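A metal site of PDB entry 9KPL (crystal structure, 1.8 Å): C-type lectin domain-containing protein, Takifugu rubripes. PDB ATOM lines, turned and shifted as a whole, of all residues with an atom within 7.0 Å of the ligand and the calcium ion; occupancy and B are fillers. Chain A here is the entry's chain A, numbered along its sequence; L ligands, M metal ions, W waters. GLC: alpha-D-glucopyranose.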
ATOM      1  N   ARG A  83      24.641 -17.160  22.473  1.00  0.00           N
ATOM      2  CA  ARG A  83      23.884 -16.837  21.258  1.00  0.00           C
ATOM      3  C   ARG A  83      22.587 -17.605  21.246  1.00  0.00           C
ATOM      4  O   ARG A  83      22.072 -17.966  20.186  1.00  0.00           O
ATOM      5  CB  ARG A  83      24.651 -17.122  19.941  1.00  0.00           C
ATOM      6  CG  ARG A  83      26.004 -16.332  19.879  1.00  0.00           C
ATOM      7  CD  ARG A  83      25.788 -14.920  19.342  1.00  0.00           C
ATOM      8  NE  ARG A  83      25.371 -13.915  20.325  1.00  0.00           N
ATOM      9  CZ  ARG A  83      25.029 -12.691  19.932  1.00  0.00           C
ATOM     10  NH1 ARG A  83      24.982 -12.373  18.629  1.00  0.00           N
ATOM     11  NH2 ARG A  83      24.665 -11.801  20.834  1.00  0.00           N
ATOM     12  N   SER A  99      16.185  -7.793  12.897  1.00  0.00           N
ATOM     13  CA  SER A  99      16.402  -7.080  11.656  1.00  0.00           C
ATOM     14  C   SER A  99      17.485  -7.799  10.849  1.00  0.00           C
ATOM     15  O   SER A  99      18.218  -8.659  11.354  1.00  0.00           O
ATOM     16  CB  SER A  99      16.750  -5.603  11.886  1.00  0.00           C
ATOM     17  OG  SER A  99      17.867  -5.409  12.760  1.00  0.00           O
ATOM     18  N   LEU A 100      17.559  -7.482   9.574  1.00  0.00           N
ATOM     19  CA  LEU A 100      18.471  -8.216   8.689  1.00  0.00           C
ATOM     20  C   LEU A 100      19.933  -8.156   9.171  1.00  0.00           C
ATOM     21  O   LEU A 100      20.466  -7.097   9.455  1.00  0.00           O
ATOM     22  CB  LEU A 100      18.340  -7.624   7.282  1.00  0.00           C
ATOM     23  CG  LEU A 100      18.885  -8.448   6.139  1.00  0.00           C
ATOM     24  CD1 LEU A 100      17.715  -9.275   5.563  1.00  0.00           C
ATOM     25  CD2 LEU A 100      19.494  -7.513   5.091  1.00  0.00           C
ATOM     26  N   GLY A 101      20.600  -9.311   9.215  1.00  0.00           N
ATOM     27  CA  GLY A 101      21.981  -9.281   9.637  1.00  0.00           C
ATOM     28  C   GLY A 101      22.171  -9.464  11.134  1.00  0.00           C
ATOM     29  O   GLY A 101      23.307  -9.680  11.590  1.00  0.00           O
ATOM     30  N   GLU A 102      21.086  -9.501  11.903  1.00  0.00           N
ATOM     31  CA  GLU A 102      21.181  -9.604  13.375  1.00  0.00           C
ATOM     32  C   GLU A 102      20.644 -10.954  13.843  1.00  0.00           C
ATOM     33  O   GLU A 102      19.831 -11.590  13.164  1.00  0.00           O
ATOM     34  CB  GLU A 102      20.362  -8.488  14.059  1.00  0.00           C
ATOM     35  CG  GLU A 102      20.661  -7.078  13.558  1.00  0.00           C
ATOM     36  CD  GLU A 102      22.066  -6.605  13.873  1.00  0.00           C
ATOM     37  OE1 GLU A 102      22.719  -7.202  14.761  1.00  0.00           O
ATOM     38  OE2 GLU A 102      22.530  -5.597  13.249  1.00  0.00           O
ATOM     39  N   PRO A 103      21.073 -11.410  15.019  1.00  0.00           N
ATOM     40  CA  PRO A 103      22.037 -10.764  15.950  1.00  0.00           C
ATOM     41  C   PRO A 103      23.472 -11.022  15.489  1.00  0.00           C
ATOM     42  O   PRO A 103      23.718 -12.035  14.794  1.00  0.00           O
ATOM     43  CB  PRO A 103      21.719 -11.417  17.309  1.00  0.00           C
ATOM     44  CG  PRO A 103      21.207 -12.856  16.926  1.00  0.00           C
ATOM     45  CD  PRO A 103      20.628 -12.739  15.494  1.00  0.00           C
ATOM     46  N   ASN A 104      24.401 -10.121  15.814  1.00  0.00           N
ATOM     47  CA  ASN A 104      25.709 -10.233  15.170  1.00  0.00           C
ATOM     48  C   ASN A 104      26.930  -9.941  16.036  1.00  0.00           C
ATOM     49  O   ASN A 104      28.041 -10.006  15.482  1.00  0.00           O
ATOM     50  CB  ASN A 104      25.749  -9.313  13.931  1.00  0.00           C
ATOM     51  CG  ASN A 104      25.727  -7.822  14.302  1.00  0.00           C
ATOM     52  OD1 ASN A 104      25.568  -7.479  15.464  1.00  0.00           O
ATOM     53  ND2 ASN A 104      25.905  -6.926  13.296  1.00  0.00           N
ATOM     54  N   ASN A 105      26.798  -9.606  17.348  1.00  0.00           N
ATOM     55  CA  ASN A 105      27.983  -9.272  18.167  1.00  0.00           C
ATOM     56  C   ASN A 105      28.914  -8.344  17.379  1.00  0.00           C
ATOM     57  O   ASN A 105      30.116  -8.613  17.225  1.00  0.00           O
ATOM     58  CB  ASN A 105      28.762 -10.516  18.607  1.00  0.00           C
ATOM     59  CG  ASN A 105      28.179 -11.120  19.882  1.00  0.00           C
ATOM     60  OD1 ASN A 105      27.686 -10.386  20.757  1.00  0.00           O
ATOM     61  ND2 ASN A 105      28.229 -12.466  19.999  1.00  0.00           N
ATOM     62  N   TYR A 106      28.317  -7.269  16.844  1.00  0.00           N
ATOM     63  CA  TYR A 106      28.953  -6.322  15.915  1.00  0.00           C
ATOM     64  C   TYR A 106      30.372  -5.962  16.313  1.00  0.00           C
ATOM     65  O   TYR A 106      30.623  -5.571  17.454  1.00  0.00           O
ATOM     66  CB  TYR A 106      28.157  -5.028  15.886  1.00  0.00           C
ATOM     67  CG  TYR A 106      28.504  -4.072  14.739  1.00  0.00           C
ATOM     68  CD1 TYR A 106      28.411  -4.470  13.407  1.00  0.00           C
ATOM     69  CD2 TYR A 106      28.894  -2.758  15.022  1.00  0.00           C
ATOM     70  CE1 TYR A 106      28.684  -3.561  12.361  1.00  0.00           C
ATOM     71  CE2 TYR A 106      29.148  -1.842  13.967  1.00  0.00           C
ATOM     72  CZ  TYR A 106      29.066  -2.274  12.666  1.00  0.00           C
ATOM     73  OH  TYR A 106      29.319  -1.410  11.641  1.00  0.00           O
ATOM     74  N   GLU A 107      31.283  -6.041  15.343  1.00  0.00           N
ATOM     75  CA  GLU A 107      32.676  -5.631  15.557  1.00  0.00           C
ATOM     76  C   GLU A 107      33.324  -6.373  16.717  1.00  0.00           C
ATOM     77  O   GLU A 107      34.240  -5.866  17.365  1.00  0.00           O
ATOM     78  CB  GLU A 107      32.771  -4.111  15.786  1.00  0.00           C
ATOM     79  CG  GLU A 107      32.433  -3.317  14.522  1.00  0.00           C
ATOM     80  CD  GLU A 107      32.817  -1.870  14.685  1.00  0.00           C
ATOM     81  OE1 GLU A 107      32.312  -1.191  15.609  1.00  0.00           O
ATOM     82  OE2 GLU A 107      33.663  -1.407  13.907  1.00  0.00           O
ATOM     83  N   ARG A 109      32.096  -7.010  19.712  1.00  0.00           N
ATOM     84  CA  ARG A 109      31.619  -6.559  21.018  1.00  0.00           C
ATOM     85  C   ARG A 109      30.577  -7.510  21.573  1.00  0.00           C
ATOM     86  O   ARG A 109      29.836  -8.151  20.823  1.00  0.00           O
ATOM     87  CB  ARG A 109      30.963  -5.163  20.944  1.00  0.00           C
ATOM     88  CG  ARG A 109      31.836  -4.189  20.181  1.00  0.00           C
ATOM     89  CD  ARG A 109      31.378  -2.753  20.122  1.00  0.00           C
ATOM     90  NE  ARG A 109      30.087  -2.580  19.457  1.00  0.00           N
ATOM     91  CZ  ARG A 109      29.592  -1.391  19.110  1.00  0.00           C
ATOM     92  NH1 ARG A 109      30.271  -0.282  19.307  1.00  0.00           N
ATOM     93  NH2 ARG A 109      28.402  -1.332  18.544  1.00  0.00           N
ATOM     94  N   GLU A 111      27.293  -8.181  22.582  1.00  0.00           N
ATOM     95  CA  GLU A 111      25.978  -7.561  22.396  1.00  0.00           C
ATOM     96  C   GLU A 111      24.911  -8.481  22.969  1.00  0.00           C
ATOM     97  O   GLU A 111      24.380  -9.321  22.276  1.00  0.00           O
ATOM     98  CB  GLU A 111      25.717  -7.164  20.944  1.00  0.00           C
ATOM     99  CG  GLU A 111      26.773  -6.180  20.341  1.00  0.00           C
ATOM    100  CD  GLU A 111      26.230  -5.547  19.118  1.00  0.00           C
ATOM    101  OE1 GLU A 111      25.868  -6.303  18.202  1.00  0.00           O
ATOM    102  OE2 GLU A 111      26.266  -4.297  19.012  1.00  0.00           O
ATOM    103  N   GLU A 115      17.490  -4.534  21.547  1.00  0.00           N
ATOM    104  CA  GLU A 115      16.660  -3.359  21.303  1.00  0.00           C
ATOM    105  C   GLU A 115      15.813  -3.545  20.040  1.00  0.00           C
ATOM    106  O   GLU A 115      16.156  -4.312  19.130  1.00  0.00           O
ATOM    107  CB  GLU A 115      17.572  -2.119  21.114  1.00  0.00           C
ATOM    108  CG  GLU A 115      18.411  -2.227  19.798  1.00  0.00           C
ATOM    109  CD  GLU A 115      19.347  -1.013  19.540  1.00  0.00           C
ATOM    110  OE1 GLU A 115      19.358  -0.059  20.359  1.00  0.00           O
ATOM    111  OE2 GLU A 115      20.061  -1.048  18.525  1.00  0.00           O
ATOM    112  N   ILE A 117      15.036  -1.414  16.877  1.00  0.00           N
ATOM    113  CA  ILE A 117      15.713  -0.281  16.256  1.00  0.00           C
ATOM    114  C   ILE A 117      14.698   0.530  15.475  1.00  0.00           C
ATOM    115  O   ILE A 117      13.616   0.069  15.107  1.00  0.00           O
ATOM    116  CB  ILE A 117      16.859  -0.719  15.357  1.00  0.00           C
ATOM    117  CG1 ILE A 117      16.301  -1.273  14.053  1.00  0.00           C
ATOM    118  CG2 ILE A 117      17.749  -1.685  16.068  1.00  0.00           C
ATOM    119  CD1 ILE A 117      17.328  -2.036  13.255  1.00  0.00           C
ATOM    120  N   ARG A 119      15.339   2.616  12.217  1.00  0.00           N
ATOM    121  CA  ARG A 119      16.316   3.040  11.229  1.00  0.00           C
ATOM    122  C   ARG A 119      15.679   3.036   9.850  1.00  0.00           C
ATOM    123  O   ARG A 119      14.736   2.283   9.577  1.00  0.00           O
ATOM    124  CB  ARG A 119      17.586   2.149  11.216  1.00  0.00           C
ATOM    125  CG  ARG A 119      18.468   2.318  12.444  1.00  0.00           C
ATOM    126  CD  ARG A 119      19.641   1.334  12.382  1.00  0.00           C
ATOM    127  NE  ARG A 119      20.564   1.610  11.286  1.00  0.00           N
ATOM    128  CZ  ARG A 119      21.712   2.268  11.414  1.00  0.00           C
ATOM    129  NH1 ARG A 119      22.136   2.672  12.603  1.00  0.00           N
ATOM    130  NH2 ARG A 119      22.444   2.517  10.330  1.00  0.00           N
ATOM    131  N   LYS A 122      15.974  -0.400   7.866  1.00  0.00           N
ATOM    132  CA  LYS A 122      16.368  -1.483   8.779  1.00  0.00           C
ATOM    133  C   LYS A 122      15.497  -1.356  10.021  1.00  0.00           C
ATOM    134  O   LYS A 122      15.746  -0.478  10.854  1.00  0.00           O
ATOM    135  CB  LYS A 122      17.843  -1.392   9.145  1.00  0.00           C
ATOM    136  CG  LYS A 122      18.491  -2.743   9.394  1.00  0.00           C
ATOM    137  CD  LYS A 122      19.904  -2.630   9.978  1.00  0.00           C
ATOM    138  CE  LYS A 122      20.236  -3.849  10.889  1.00  0.00           C
ATOM    139  NZ  LYS A 122      20.706  -3.464  12.288  1.00  0.00           N
ATOM    140  N   TRP A 125      14.629  -6.216  15.491  1.00  0.00           N
ATOM    141  CA  TRP A 125      15.457  -6.252  16.692  1.00  0.00           C
ATOM    142  C   TRP A 125      16.949  -6.257  16.345  1.00  0.00           C
ATOM    143  O   TRP A 125      17.367  -6.699  15.260  1.00  0.00           O
ATOM    144  CB  TRP A 125      15.213  -7.517  17.485  1.00  0.00           C
ATOM    145  CG  TRP A 125      13.751  -7.815  17.830  1.00  0.00           C
ATOM    146  CD1 TRP A 125      12.676  -6.963  17.835  1.00  0.00           C
ATOM    147  CD2 TRP A 125      13.272  -9.097  18.244  1.00  0.00           C
ATOM    148  NE1 TRP A 125      11.520  -7.675  18.279  1.00  0.00           N
ATOM    149  CE2 TRP A 125      11.889  -8.982  18.505  1.00  0.00           C
ATOM    150  CE3 TRP A 125      13.900 -10.336  18.452  1.00  0.00           C
ATOM    151  CZ2 TRP A 125      11.142 -10.058  18.951  1.00  0.00           C
ATOM    152  CZ3 TRP A 125      13.151 -11.416  18.845  1.00  0.00           C
ATOM    153  CH2 TRP A 125      11.785 -11.275  19.078  1.00  0.00           C
ATOM    154  N   ASN A 126      17.743  -5.837  17.327  1.00  0.00           N
ATOM    155  CA  ASN A 126      19.195  -5.740  17.164  1.00  0.00           C
ATOM    156  C   ASN A 126      19.802  -6.115  18.511  1.00  0.00           C
ATOM    157  O   ASN A 126      19.296  -5.655  19.563  1.00  0.00           O
ATOM    158  CB  ASN A 126      19.642  -4.322  16.743  1.00  0.00           C
ATOM    159  CG  ASN A 126      21.162  -4.168  16.837  1.00  0.00           C
ATOM    160  OD1 ASN A 126      21.905  -5.022  16.292  1.00  0.00           O
ATOM    161  ND2 ASN A 126      21.637  -3.092  17.494  1.00  0.00           N
ATOM    162  N   ASP A 127      20.803  -6.995  18.507  1.00  0.00           N
ATOM    163  CA  ASP A 127      21.559  -7.164  19.742  1.00  0.00           C
ATOM    164  C   ASP A 127      22.533  -5.988  19.933  1.00  0.00           C
ATOM    165  O   ASP A 127      23.162  -5.508  18.967  1.00  0.00           O
ATOM    166  CB  ASP A 127      22.301  -8.519  19.797  1.00  0.00           C
ATOM    167  CG  ASP A 127      23.317  -8.732  18.631  1.00  0.00           C
ATOM    168  OD1 ASP A 127      23.128  -8.156  17.529  1.00  0.00           O
ATOM    169  OD2 ASP A 127      24.256  -9.516  18.813  1.00  0.00           O
ATOM    170  N   LEU A 128      22.611  -5.507  21.179  1.00  0.00           N
ATOM    171  CA  LEU A 128      23.422  -4.326  21.536  1.00  0.00           C
ATOM    172  C   LEU A 128      24.103  -4.514  22.886  1.00  0.00           C
ATOM    173  O   LEU A 128      23.655  -5.263  23.737  1.00  0.00           O
ATOM    174  CB  LEU A 128      22.505  -3.068  21.610  1.00  0.00           C
ATOM    175  CG  LEU A 128      23.228  -1.722  21.588  1.00  0.00           C
ATOM    176  CD1 LEU A 128      23.895  -1.664  20.264  1.00  0.00           C
ATOM    177  CD2 LEU A 128      22.229  -0.554  21.802  1.00  0.00           C
ATOM    178  N   VAL A 129      25.246  -3.819  23.074  1.00  0.00           N
ATOM    179  CA  VAL A 129      25.903  -3.782  24.398  1.00  0.00           C
ATOM    180  C   VAL A 129      24.896  -3.355  25.482  1.00  0.00           C
ATOM    181  O   VAL A 129      24.199  -2.330  25.360  1.00  0.00           O
ATOM    182  CB  VAL A 129      27.077  -2.821  24.351  1.00  0.00           C
ATOM    183  CG1 VAL A 129      27.740  -2.813  25.698  1.00  0.00           C
ATOM    184  CG2 VAL A 129      28.043  -3.270  23.262  1.00  0.00           C
ATOM    185  N   PHE A 132      24.983   0.290  26.898  1.00  0.00           N
ATOM    186  CA  PHE A 132      24.540   1.439  26.119  1.00  0.00           C
ATOM    187  C   PHE A 132      23.139   1.870  26.580  1.00  0.00           C
ATOM    188  O   PHE A 132      22.454   1.125  27.265  1.00  0.00           O
ATOM    189  CB  PHE A 132      24.469   1.119  24.619  1.00  0.00           C
ATOM    190  CG  PHE A 132      25.831   0.893  23.962  1.00  0.00           C
ATOM    191  CD1 PHE A 132      27.003   0.907  24.723  1.00  0.00           C
ATOM    192  CD2 PHE A 132      25.927   0.676  22.571  1.00  0.00           C
ATOM    193  CE1 PHE A 132      28.264   0.672  24.098  1.00  0.00           C
ATOM    194  CE2 PHE A 132      27.190   0.444  21.932  1.00  0.00           C
ATOM    195  CZ  PHE A 132      28.348   0.436  22.707  1.00  0.00           C
HETATM  196  C1  GLC L   1      25.220  -1.048  13.854  1.00  0.00           C
HETATM  197  C2  GLC L   1      25.050  -2.607  13.558  1.00  0.00           C
HETATM  198  C3  GLC L   1      24.408  -3.349  14.800  1.00  0.00           C
HETATM  199  C4  GLC L   1      25.244  -2.954  16.087  1.00  0.00           C
HETATM  200  C5  GLC L   1      25.124  -1.400  16.213  1.00  0.00           C
HETATM  201  C6  GLC L   1      25.717  -0.921  17.496  1.00  0.00           C
HETATM  202  O1  GLC L   1      23.936  -0.540  13.873  1.00  0.00           O
HETATM  203  O2  GLC L   1      24.124  -2.755  12.507  1.00  0.00           O
HETATM  204  O3  GLC L   1      24.529  -4.713  14.614  1.00  0.00           O
HETATM  205  O4  GLC L   1      24.721  -3.677  17.222  1.00  0.00           O
HETATM  206  O5  GLC L   1      25.748  -0.772  15.145  1.00  0.00           O
HETATM  207  O6  GLC L   1      26.011   0.444  17.287  1.00  0.00           O
HETATM  208 CA    CA M   1      23.987  -6.069  16.689  1.00  0.00          CA
HETATM  209  O   HOH W   1      24.446   1.787  18.548  1.00  0.00           O
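The guanidinium group (NH2) of Arg 109 lies close to an oxygen (O6) of the ligand (3.2 Å).
NZ of Lys 122 is in hydrogen-bond range of O2 of the ligand (3.5 Å).
OD2 of Asp 127 is in salt-bridge range of NH1 of Arg 83, 3.0 Å away.
The side-chain carboxylate of Glu 115 is in hydrogen-bond range of the side-chain amide nitrogen of Asn 126, at 2.8 Å.
The backbone NH of Glu 111 is in hydrogen-bond range of the side-chain amide oxygen of Asn 105.
O of Arg 109 sits close to OD1 of Asn 105 (3.1 Å).
The side-chain carboxylate of Glu 111 sits close to the backbone NH of Tyr 106 (3.0 Å).
OE2 of Glu 111 is in salt-bridge range of NH2 of Arg 109 (3.7 Å).
NZ of Lys 122 lies within salt-bridge range of OE2 of Glu 102 (3.0 Å).
The side-chain hydroxyl (OG) of Ser 99 lies close to the side-chain amino group (NZ) of Lys 122 (3.5 Å).
The calcium ion is bound by the side-chain amide oxygen of Asn 126, the side-chain carboxylate of Asp 127, the side-chain carboxylate of Glu 111, the side-chain amide oxygen of Asn 104, the backbone carbonyl oxygen of Asp 127, an oxygen (O3) of the ligand, an oxygen (O4) of the ligand and the side-chain carboxylate of Glu 102.
The calcium ion has eight donor atoms within binding distance.
The nearest printed residue that does not touch the calcium ion is Tyr 106 (4.4 Å).
Merely in contact with the ligand: Tyr 106, Arg 119 and Leu 128.
Hydrophobic or aromatic side chains within 4 Å of the ligand: Tyr 106 and Leu 128.
The nearest printed residue that does not touch the ligand is Phe 132 (4.8 Å).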
